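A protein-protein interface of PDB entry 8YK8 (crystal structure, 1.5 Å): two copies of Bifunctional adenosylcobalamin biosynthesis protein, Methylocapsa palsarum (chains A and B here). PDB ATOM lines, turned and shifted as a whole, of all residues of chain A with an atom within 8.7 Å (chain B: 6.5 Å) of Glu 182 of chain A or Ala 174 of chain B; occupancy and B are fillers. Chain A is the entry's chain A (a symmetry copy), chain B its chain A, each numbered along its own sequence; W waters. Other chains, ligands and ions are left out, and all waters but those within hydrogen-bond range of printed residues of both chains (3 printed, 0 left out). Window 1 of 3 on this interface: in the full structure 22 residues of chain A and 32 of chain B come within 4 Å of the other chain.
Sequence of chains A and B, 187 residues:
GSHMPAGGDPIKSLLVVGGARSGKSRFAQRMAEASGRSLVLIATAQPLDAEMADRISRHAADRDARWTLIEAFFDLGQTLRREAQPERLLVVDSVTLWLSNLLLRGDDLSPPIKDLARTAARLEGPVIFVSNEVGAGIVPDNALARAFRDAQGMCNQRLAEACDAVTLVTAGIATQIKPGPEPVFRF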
ATOM      1  N   ALA A 160      -6.314  28.679 -13.145  1.00  0.00           N
ATOM      2  CA  ALA A 160      -7.440  29.180 -13.952  1.00  0.00           C
ATOM      3  C   ALA A 160      -8.746  28.895 -13.206  1.00  0.00           C
ATOM      4  O   ALA A 160      -9.640  29.739 -13.241  1.00  0.00           O
ATOM      5  CB  ALA A 160      -7.428  28.547 -15.301  1.00  0.00           C
ATOM      6  N   GLU A 161      -8.842  27.751 -12.564  1.00  0.00           N
ATOM      7  CA  GLU A 161     -10.057  27.385 -11.778  1.00  0.00           C
ATOM      8  C   GLU A 161     -10.189  28.359 -10.617  1.00  0.00           C
ATOM      9  O   GLU A 161     -11.329  28.810 -10.346  1.00  0.00           O
ATOM     10  CB  GLU A 161      -9.883  25.939 -11.320  1.00  0.00           C
ATOM     11  CG  GLU A 161     -11.054  25.351 -10.548  1.00  0.00           C
ATOM     12  CD  GLU A 161     -10.801  23.867 -10.268  1.00  0.00           C
ATOM     13  OE1 GLU A 161     -11.800  23.125 -10.156  1.00  0.00           O
ATOM     14  OE2 GLU A 161      -9.585  23.417 -10.199  1.00  0.00           O
ATOM     15  N   ILE A 177     -10.591  34.483 -21.691  1.00  0.00           N
ATOM     16  CA  ILE A 177     -11.226  33.157 -21.791  1.00  0.00           C
ATOM     17  C   ILE A 177     -12.012  32.834 -20.508  1.00  0.00           C
ATOM     18  O   ILE A 177     -12.779  31.866 -20.550  1.00  0.00           O
ATOM     19  CB  ILE A 177     -10.208  32.068 -22.159  1.00  0.00           C
ATOM     20  CG1 ILE A 177      -9.128  31.856 -21.095  1.00  0.00           C
ATOM     21  CG2 ILE A 177      -9.632  32.349 -23.526  1.00  0.00           C
ATOM     22  CD1 ILE A 177      -8.304  30.574 -21.320  1.00  0.00           C
ATOM     23  N   LYS A 178     -11.839  33.590 -19.436  1.00  0.00           N
ATOM     24  CA  LYS A 178     -12.648  33.456 -18.210  1.00  0.00           C
ATOM     25  C   LYS A 178     -12.807  34.847 -17.647  1.00  0.00           C
ATOM     26  O   LYS A 178     -11.842  35.568 -17.591  1.00  0.00           O
ATOM     27  CB  LYS A 178     -12.022  32.519 -17.189  1.00  0.00           C
ATOM     28  CG  LYS A 178     -12.814  32.358 -15.896  1.00  0.00           C
ATOM     29  CD  LYS A 178     -12.142  31.549 -14.865  1.00  0.00           C
ATOM     30  CE  LYS A 178     -12.993  31.303 -13.634  1.00  0.00           C
ATOM     31  NZ  LYS A 178     -12.346  30.537 -12.582  1.00  0.00           N
ATOM     32  N   PRO A 179     -14.013  35.291 -17.242  1.00  0.00           N
ATOM     33  CA  PRO A 179     -15.261  34.547 -17.416  1.00  0.00           C
ATOM     34  C   PRO A 179     -15.644  34.305 -18.881  1.00  0.00           C
ATOM     35  O   PRO A 179     -15.237  35.018 -19.767  1.00  0.00           O
ATOM     36  CB  PRO A 179     -16.294  35.477 -16.734  1.00  0.00           C
ATOM     37  CG  PRO A 179     -15.668  36.815 -16.721  1.00  0.00           C
ATOM     38  CD  PRO A 179     -14.174  36.598 -16.604  1.00  0.00           C
ATOM     39  N   GLY A 180     -16.422  33.258 -19.115  1.00  0.00           N
ATOM     40  CA  GLY A 180     -16.899  32.903 -20.460  1.00  0.00           C
ATOM     41  C   GLY A 180     -17.639  31.586 -20.367  1.00  0.00           C
ATOM     42  O   GLY A 180     -17.267  30.733 -19.587  1.00  0.00           O
ATOM     43  N   PRO A 181     -18.758  31.423 -21.088  1.00  0.00           N
ATOM     44  CA  PRO A 181     -19.463  30.164 -21.003  1.00  0.00           C
ATOM     45  C   PRO A 181     -18.650  29.108 -21.737  1.00  0.00           C
ATOM     46  O   PRO A 181     -18.303  29.318 -22.864  1.00  0.00           O
ATOM     47  CB  PRO A 181     -20.827  30.428 -21.665  1.00  0.00           C
ATOM     48  CG  PRO A 181     -20.725  31.799 -22.310  1.00  0.00           C
ATOM     49  CD  PRO A 181     -19.410  32.439 -21.923  1.00  0.00           C
ATOM     50  N   GLU A 182     -18.448  27.983 -21.092  1.00  0.00           N
ATOM     51  CA  GLU A 182     -17.735  26.872 -21.773  1.00  0.00           C
ATOM     52  C   GLU A 182     -18.738  26.068 -22.599  1.00  0.00           C
ATOM     53  O   GLU A 182     -19.910  25.929 -22.254  1.00  0.00           O
ATOM     54  CB  GLU A 182     -16.874  26.092 -20.797  1.00  0.00           C
ATOM     55  CG  GLU A 182     -15.589  26.836 -20.423  1.00  0.00           C
ATOM     56  CD  GLU A 182     -14.677  26.042 -19.512  1.00  0.00           C
ATOM     57  OE1 GLU A 182     -14.657  26.318 -18.282  1.00  0.00           O
ATOM     58  OE2 GLU A 182     -14.190  25.041 -19.978  1.00  0.00           O
ATOM     59  N   PRO A 183     -18.303  25.509 -23.741  1.00  0.00           N
ATOM     60  CA  PRO A 183     -19.179  24.813 -24.654  1.00  0.00           C
ATOM     61  C   PRO A 183     -19.713  23.510 -24.058  1.00  0.00           C
ATOM     62  O   PRO A 183     -19.046  22.881 -23.230  1.00  0.00           O
ATOM     63  CB  PRO A 183     -18.340  24.537 -25.924  1.00  0.00           C
ATOM     64  CG  PRO A 183     -16.919  24.816 -25.550  1.00  0.00           C
ATOM     65  CD  PRO A 183     -16.919  25.585 -24.256  1.00  0.00           C
ATOM     66  N   VAL A 184     -20.925  23.159 -24.466  1.00  0.00           N
ATOM     67  CA  VAL A 184     -21.617  21.904 -24.083  1.00  0.00           C
ATOM     68  C   VAL A 184     -22.076  21.261 -25.382  1.00  0.00           C
ATOM     69  O   VAL A 184     -22.579  21.983 -26.273  1.00  0.00           O
ATOM     70  CB  VAL A 184     -22.811  22.180 -23.135  1.00  0.00           C
ATOM     71  CG1 VAL A 184     -23.392  20.900 -22.572  1.00  0.00           C
ATOM     72  CG2 VAL A 184     -22.420  23.083 -22.002  1.00  0.00           C
ATOM     73  N   PHE A 185     -21.934  19.952 -25.466  1.00  0.00           N
ATOM     74  CA  PHE A 185     -22.378  19.149 -26.624  1.00  0.00           C
ATOM     75  C   PHE A 185     -23.253  18.000 -26.128  1.00  0.00           C
ATOM     76  O   PHE A 185     -22.902  17.334 -25.101  1.00  0.00           O
ATOM     77  CB  PHE A 185     -21.159  18.732 -27.447  1.00  0.00           C
ATOM     78  CG  PHE A 185     -20.330  19.893 -27.930  1.00  0.00           C
ATOM     79  CD1 PHE A 185     -20.762  20.711 -28.955  1.00  0.00           C
ATOM     80  CD2 PHE A 185     -19.131  20.187 -27.311  1.00  0.00           C
ATOM     81  CE1 PHE A 185     -19.984  21.778 -29.384  1.00  0.00           C
ATOM     82  CE2 PHE A 185     -18.369  21.256 -27.724  1.00  0.00           C
ATOM     83  CZ  PHE A 185     -18.775  22.040 -28.776  1.00  0.00           C
ATOM     84  N   PHE B  27     -11.918  17.380 -19.955  1.00  0.00           N
ATOM     85  CA  PHE B  27     -13.033  18.020 -20.659  1.00  0.00           C
ATOM     86  C   PHE B  27     -13.811  16.973 -21.445  1.00  0.00           C
ATOM     87  O   PHE B  27     -15.037  16.873 -21.319  1.00  0.00           O
ATOM     88  CB  PHE B  27     -12.538  19.142 -21.569  1.00  0.00           C
ATOM     89  CG  PHE B  27     -13.617  19.771 -22.411  1.00  0.00           C
ATOM     90  CD1 PHE B  27     -14.562  20.628 -21.840  1.00  0.00           C
ATOM     91  CD2 PHE B  27     -13.731  19.465 -23.745  1.00  0.00           C
ATOM     92  CE1 PHE B  27     -15.578  21.165 -22.609  1.00  0.00           C
ATOM     93  CE2 PHE B  27     -14.725  20.032 -24.520  1.00  0.00           C
ATOM     94  CZ  PHE B  27     -15.675  20.845 -23.956  1.00  0.00           C
ATOM     95  N   ARG B  30     -15.577  14.445 -18.977  1.00  0.00           N
ATOM     96  CA  ARG B  30     -16.765  14.886 -18.208  1.00  0.00           C
ATOM     97  C   ARG B  30     -17.839  15.172 -19.258  1.00  0.00           C
ATOM     98  O   ARG B  30     -19.010  14.826 -18.903  1.00  0.00           O
ATOM     99  CB  ARG B  30     -16.517  15.826 -17.020  1.00  0.00           C
ATOM    100  CG  ARG B  30     -16.498  17.328 -17.203  1.00  0.00           C
ATOM    101  CD  ARG B  30     -15.155  17.857 -17.602  1.00  0.00           C
ATOM    102  NE  ARG B  30     -15.195  19.290 -17.373  1.00  0.00           N
ATOM    103  CZ  ARG B  30     -15.743  20.165 -18.212  1.00  0.00           C
ATOM    104  NH1 ARG B  30     -16.285  19.756 -19.353  1.00  0.00           N
ATOM    105  NH2 ARG B  30     -15.719  21.453 -17.924  1.00  0.00           N
ATOM    106  N   THR B 167     -13.072  22.115 -30.230  1.00  0.00           N
ATOM    107  CA  THR B 167     -12.823  22.905 -29.034  1.00  0.00           C
ATOM    108  C   THR B 167     -11.313  22.904 -28.795  1.00  0.00           C
ATOM    109  O   THR B 167     -10.690  21.787 -28.865  1.00  0.00           O
ATOM    110  CB  THR B 167     -13.562  22.398 -27.813  1.00  0.00           C
ATOM    111  OG1 THR B 167     -13.173  21.070 -27.501  1.00  0.00           O
ATOM    112  CG2 THR B 167     -15.050  22.403 -28.023  1.00  0.00           C
ATOM    113  N   LEU B 168     -10.791  24.060 -28.489  1.00  0.00           N
ATOM    114  CA  LEU B 168      -9.408  24.197 -27.998  1.00  0.00           C
ATOM    115  C   LEU B 168      -9.476  24.292 -26.482  1.00  0.00           C
ATOM    116  O   LEU B 168     -10.224  25.129 -25.974  1.00  0.00           O
ATOM    117  CB  LEU B 168      -8.743  25.450 -28.594  1.00  0.00           C
ATOM    118  CG  LEU B 168      -7.315  25.744 -28.164  1.00  0.00           C
ATOM    119  CD1 LEU B 168      -6.423  24.596 -28.569  1.00  0.00           C
ATOM    120  CD2 LEU B 168      -6.816  27.040 -28.779  1.00  0.00           C
ATOM    121  N   VAL B 169      -8.673  23.529 -25.748  1.00  0.00           N
ATOM    122  CA  VAL B 169      -8.633  23.553 -24.275  1.00  0.00           C
ATOM    123  C   VAL B 169      -7.276  24.144 -23.885  1.00  0.00           C
ATOM    124  O   VAL B 169      -6.241  23.616 -24.283  1.00  0.00           O
ATOM    125  CB  VAL B 169      -8.882  22.195 -23.650  1.00  0.00           C
ATOM    126  CG1 VAL B 169      -8.842  22.301 -22.123  1.00  0.00           C
ATOM    127  CG2 VAL B 169     -10.225  21.613 -24.131  1.00  0.00           C
ATOM    128  N   THR B 170      -7.285  25.266 -23.175  1.00  0.00           N
ATOM    129  CA  THR B 170      -6.106  25.996 -22.702  1.00  0.00           C
ATOM    130  C   THR B 170      -6.246  26.163 -21.194  1.00  0.00           C
ATOM    131  O   THR B 170      -7.251  26.788 -20.707  1.00  0.00           O
ATOM    132  CB  THR B 170      -6.056  27.355 -23.365  1.00  0.00           C
ATOM    133  OG1 THR B 170      -7.233  28.090 -23.083  1.00  0.00           O
ATOM    134  CG2 THR B 170      -6.047  27.224 -24.837  1.00  0.00           C
ATOM    135  N   GLY B 172      -7.175  24.255 -18.966  1.00  0.00           N
ATOM    136  CA  GLY B 172      -8.409  23.624 -18.461  1.00  0.00           C
ATOM    137  C   GLY B 172      -9.663  24.306 -18.896  1.00  0.00           C
ATOM    138  O   GLY B 172     -10.765  23.838 -18.475  1.00  0.00           O
ATOM    139  N   ILE B 173      -9.570  25.339 -19.718  1.00  0.00           N
ATOM    140  CA  ILE B 173     -10.761  26.085 -20.186  1.00  0.00           C
ATOM    141  C   ILE B 173     -10.981  25.797 -21.652  1.00  0.00           C
ATOM    142  O   ILE B 173     -10.068  26.017 -22.484  1.00  0.00           O
ATOM    143  CB  ILE B 173     -10.617  27.587 -19.893  1.00  0.00           C
ATOM    144  CG1 ILE B 173     -10.567  27.844 -18.389  1.00  0.00           C
ATOM    145  CG2 ILE B 173     -11.758  28.342 -20.560  1.00  0.00           C
ATOM    146  CD1 ILE B 173     -10.235  29.260 -18.052  1.00  0.00           C
ATOM    147  N   ALA B 174     -12.196  25.395 -22.022  1.00  0.00           N
ATOM    148  CA  ALA B 174     -12.534  24.994 -23.388  1.00  0.00           C
ATOM    149  C   ALA B 174     -13.114  26.181 -24.136  1.00  0.00           C
ATOM    150  O   ALA B 174     -13.982  26.884 -23.575  1.00  0.00           O
ATOM    151  CB  ALA B 174     -13.498  23.849 -23.311  1.00  0.00           C
ATOM    152  N   THR B 175     -12.603  26.433 -25.312  1.00  0.00           N
ATOM    153  CA  THR B 175     -13.131  27.462 -26.228  1.00  0.00           C
ATOM    154  C   THR B 175     -13.565  26.750 -27.500  1.00  0.00           C
ATOM    155  O   THR B 175     -12.754  26.076 -28.144  1.00  0.00           O
ATOM    156  CB  THR B 175     -12.098  28.535 -26.483  1.00  0.00           C
ATOM    157  OG1 THR B 175     -11.777  29.193 -25.263  1.00  0.00           O
ATOM    158  CG2 THR B 175     -12.598  29.508 -27.526  1.00  0.00           C
ATOM    159  N   GLN B 176     -14.804  26.968 -27.952  1.00  0.00           N
ATOM    160  CA  GLN B 176     -15.312  26.416 -29.226  1.00  0.00           C
ATOM    161  C   GLN B 176     -14.784  27.240 -30.381  1.00  0.00           C
ATOM    162  O   GLN B 176     -14.961  28.474 -30.376  1.00  0.00           O
ATOM    163  CB  GLN B 176     -16.845  26.436 -29.256  1.00  0.00           C
ATOM    164  CG  GLN B 176     -17.415  25.872 -30.541  1.00  0.00           C
ATOM    165  CD  GLN B 176     -18.923  26.018 -30.554  1.00  0.00           C
ATOM    166  OE1 GLN B 176     -19.494  26.606 -31.480  1.00  0.00           O
ATOM    167  NE2 GLN B 176     -19.535  25.466 -29.533  1.00  0.00           N
HETATM  168  O   HOH W   1     -12.367  22.275 -19.907  1.00  0.00           O
HETATM  169  O   HOH W   2     -15.276  29.135 -23.619  1.00  0.00           O
HETATM  170  O   HOH W   3     -12.836  24.413 -16.920  1.00  0.00           O
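The backbone NH of Ala 174 of chain B sits at hydrogen-bond distance from the side-chain carboxylate of Glu 182 of chain A, at 2.9 Å.
O of Ala 160 of chain A is in hydrogen-bond range of NZ of Lys 178 of chain A (2.9 Å). O of Glu 161 of chain A is in hydrogen-bond range of NZ of Lys 178 of chain A (3.0 Å).
Among the printed residues, pairs that only touch across the chains: Ile 177 of chain A with Thr 170 of chain B (3.2 Å), Pro 183 of chain A with Ala 174 of chain B (3.3 Å), Phe 185 of chain A with Thr 167 of chain B (3.5 Å), Phe 185 of chain A with Gln 176 of chain B (3.6 Å), Glu 182 of chain A with Ile 173 of chain B (3.6 Å), Ile 177 of chain A with Ile 173 of chain B (3.7 Å), Lys 178 of chain A with Ile 173 of chain B (3.8 Å), Pro 183 of chain A with Gln 176 of chain B (3.9 Å), Pro 183 of chain A with Phe 27 of chain B (3.9 Å), Pro 183 of chain A with Thr 167 of chain B (3.9 Å), Glu 182 of chain A with Gly 172 of chain B (3.9 Å) and Ala 160 of chain A with Ile 173 of chain B (3.99 Å).
Glu 182 of chain A touches three residues of chain B. Of the printed residues of chain A, Thr 167 of chain B touches Pro 183 and Phe 185. Printed residues of chain A within 4 Å of Phe 27 of chain B: Pro 183. Printed residues of chain B within 4 Å of Ile 177 of chain A: Thr 170 and Ile 173. The nearest residue of chain B that does not touch Glu 182 of chain A is Arg 30 of chain B (4.4 Å). The nearest residue of chain A that does not touch Ala 174 of chain B is Pro 181 of chain A (5.0 Å). The nearest printed residue of chain A that does not touch Thr 167 of chain B is Val 184 of chain A (6.9 Å).
Of the 11 printed residues of chain A, 6 touch a printed residue of chain B. Printed residues of chain A that touch a printed residue of chain B: Ala 160, Ile 177, Lys 178, Glu 182, Pro 183 and Phe 185. Hydrophobic or aromatic side chains of chain B that line the printed part of chain A: Phe 27, Ile 173 and Ala 174. Among the printed residues, no Asp or Glu carboxylate lies within 4 Å of a Lys or Arg side-chain nitrogen of the other chain.
No position is printed for both chains.
Water W2 lies within hydrogen-bond range of the backbone carbonyl oxygen of Ala 174 of chain B (2.6 Å) and the backbone carbonyl oxygen of Pro 181 of chain A (3.1 Å). Water W3 lies within hydrogen-bond range of the backbone carbonyl oxygen of Gly 172 of chain B and the side-chain carboxylate of Glu 182 of chain A. Water W1 lies within hydrogen-bond range of the backbone carbonyl oxygen of Gly 172 of chain B and the side-chain carboxylate of Glu 182 of chain A.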
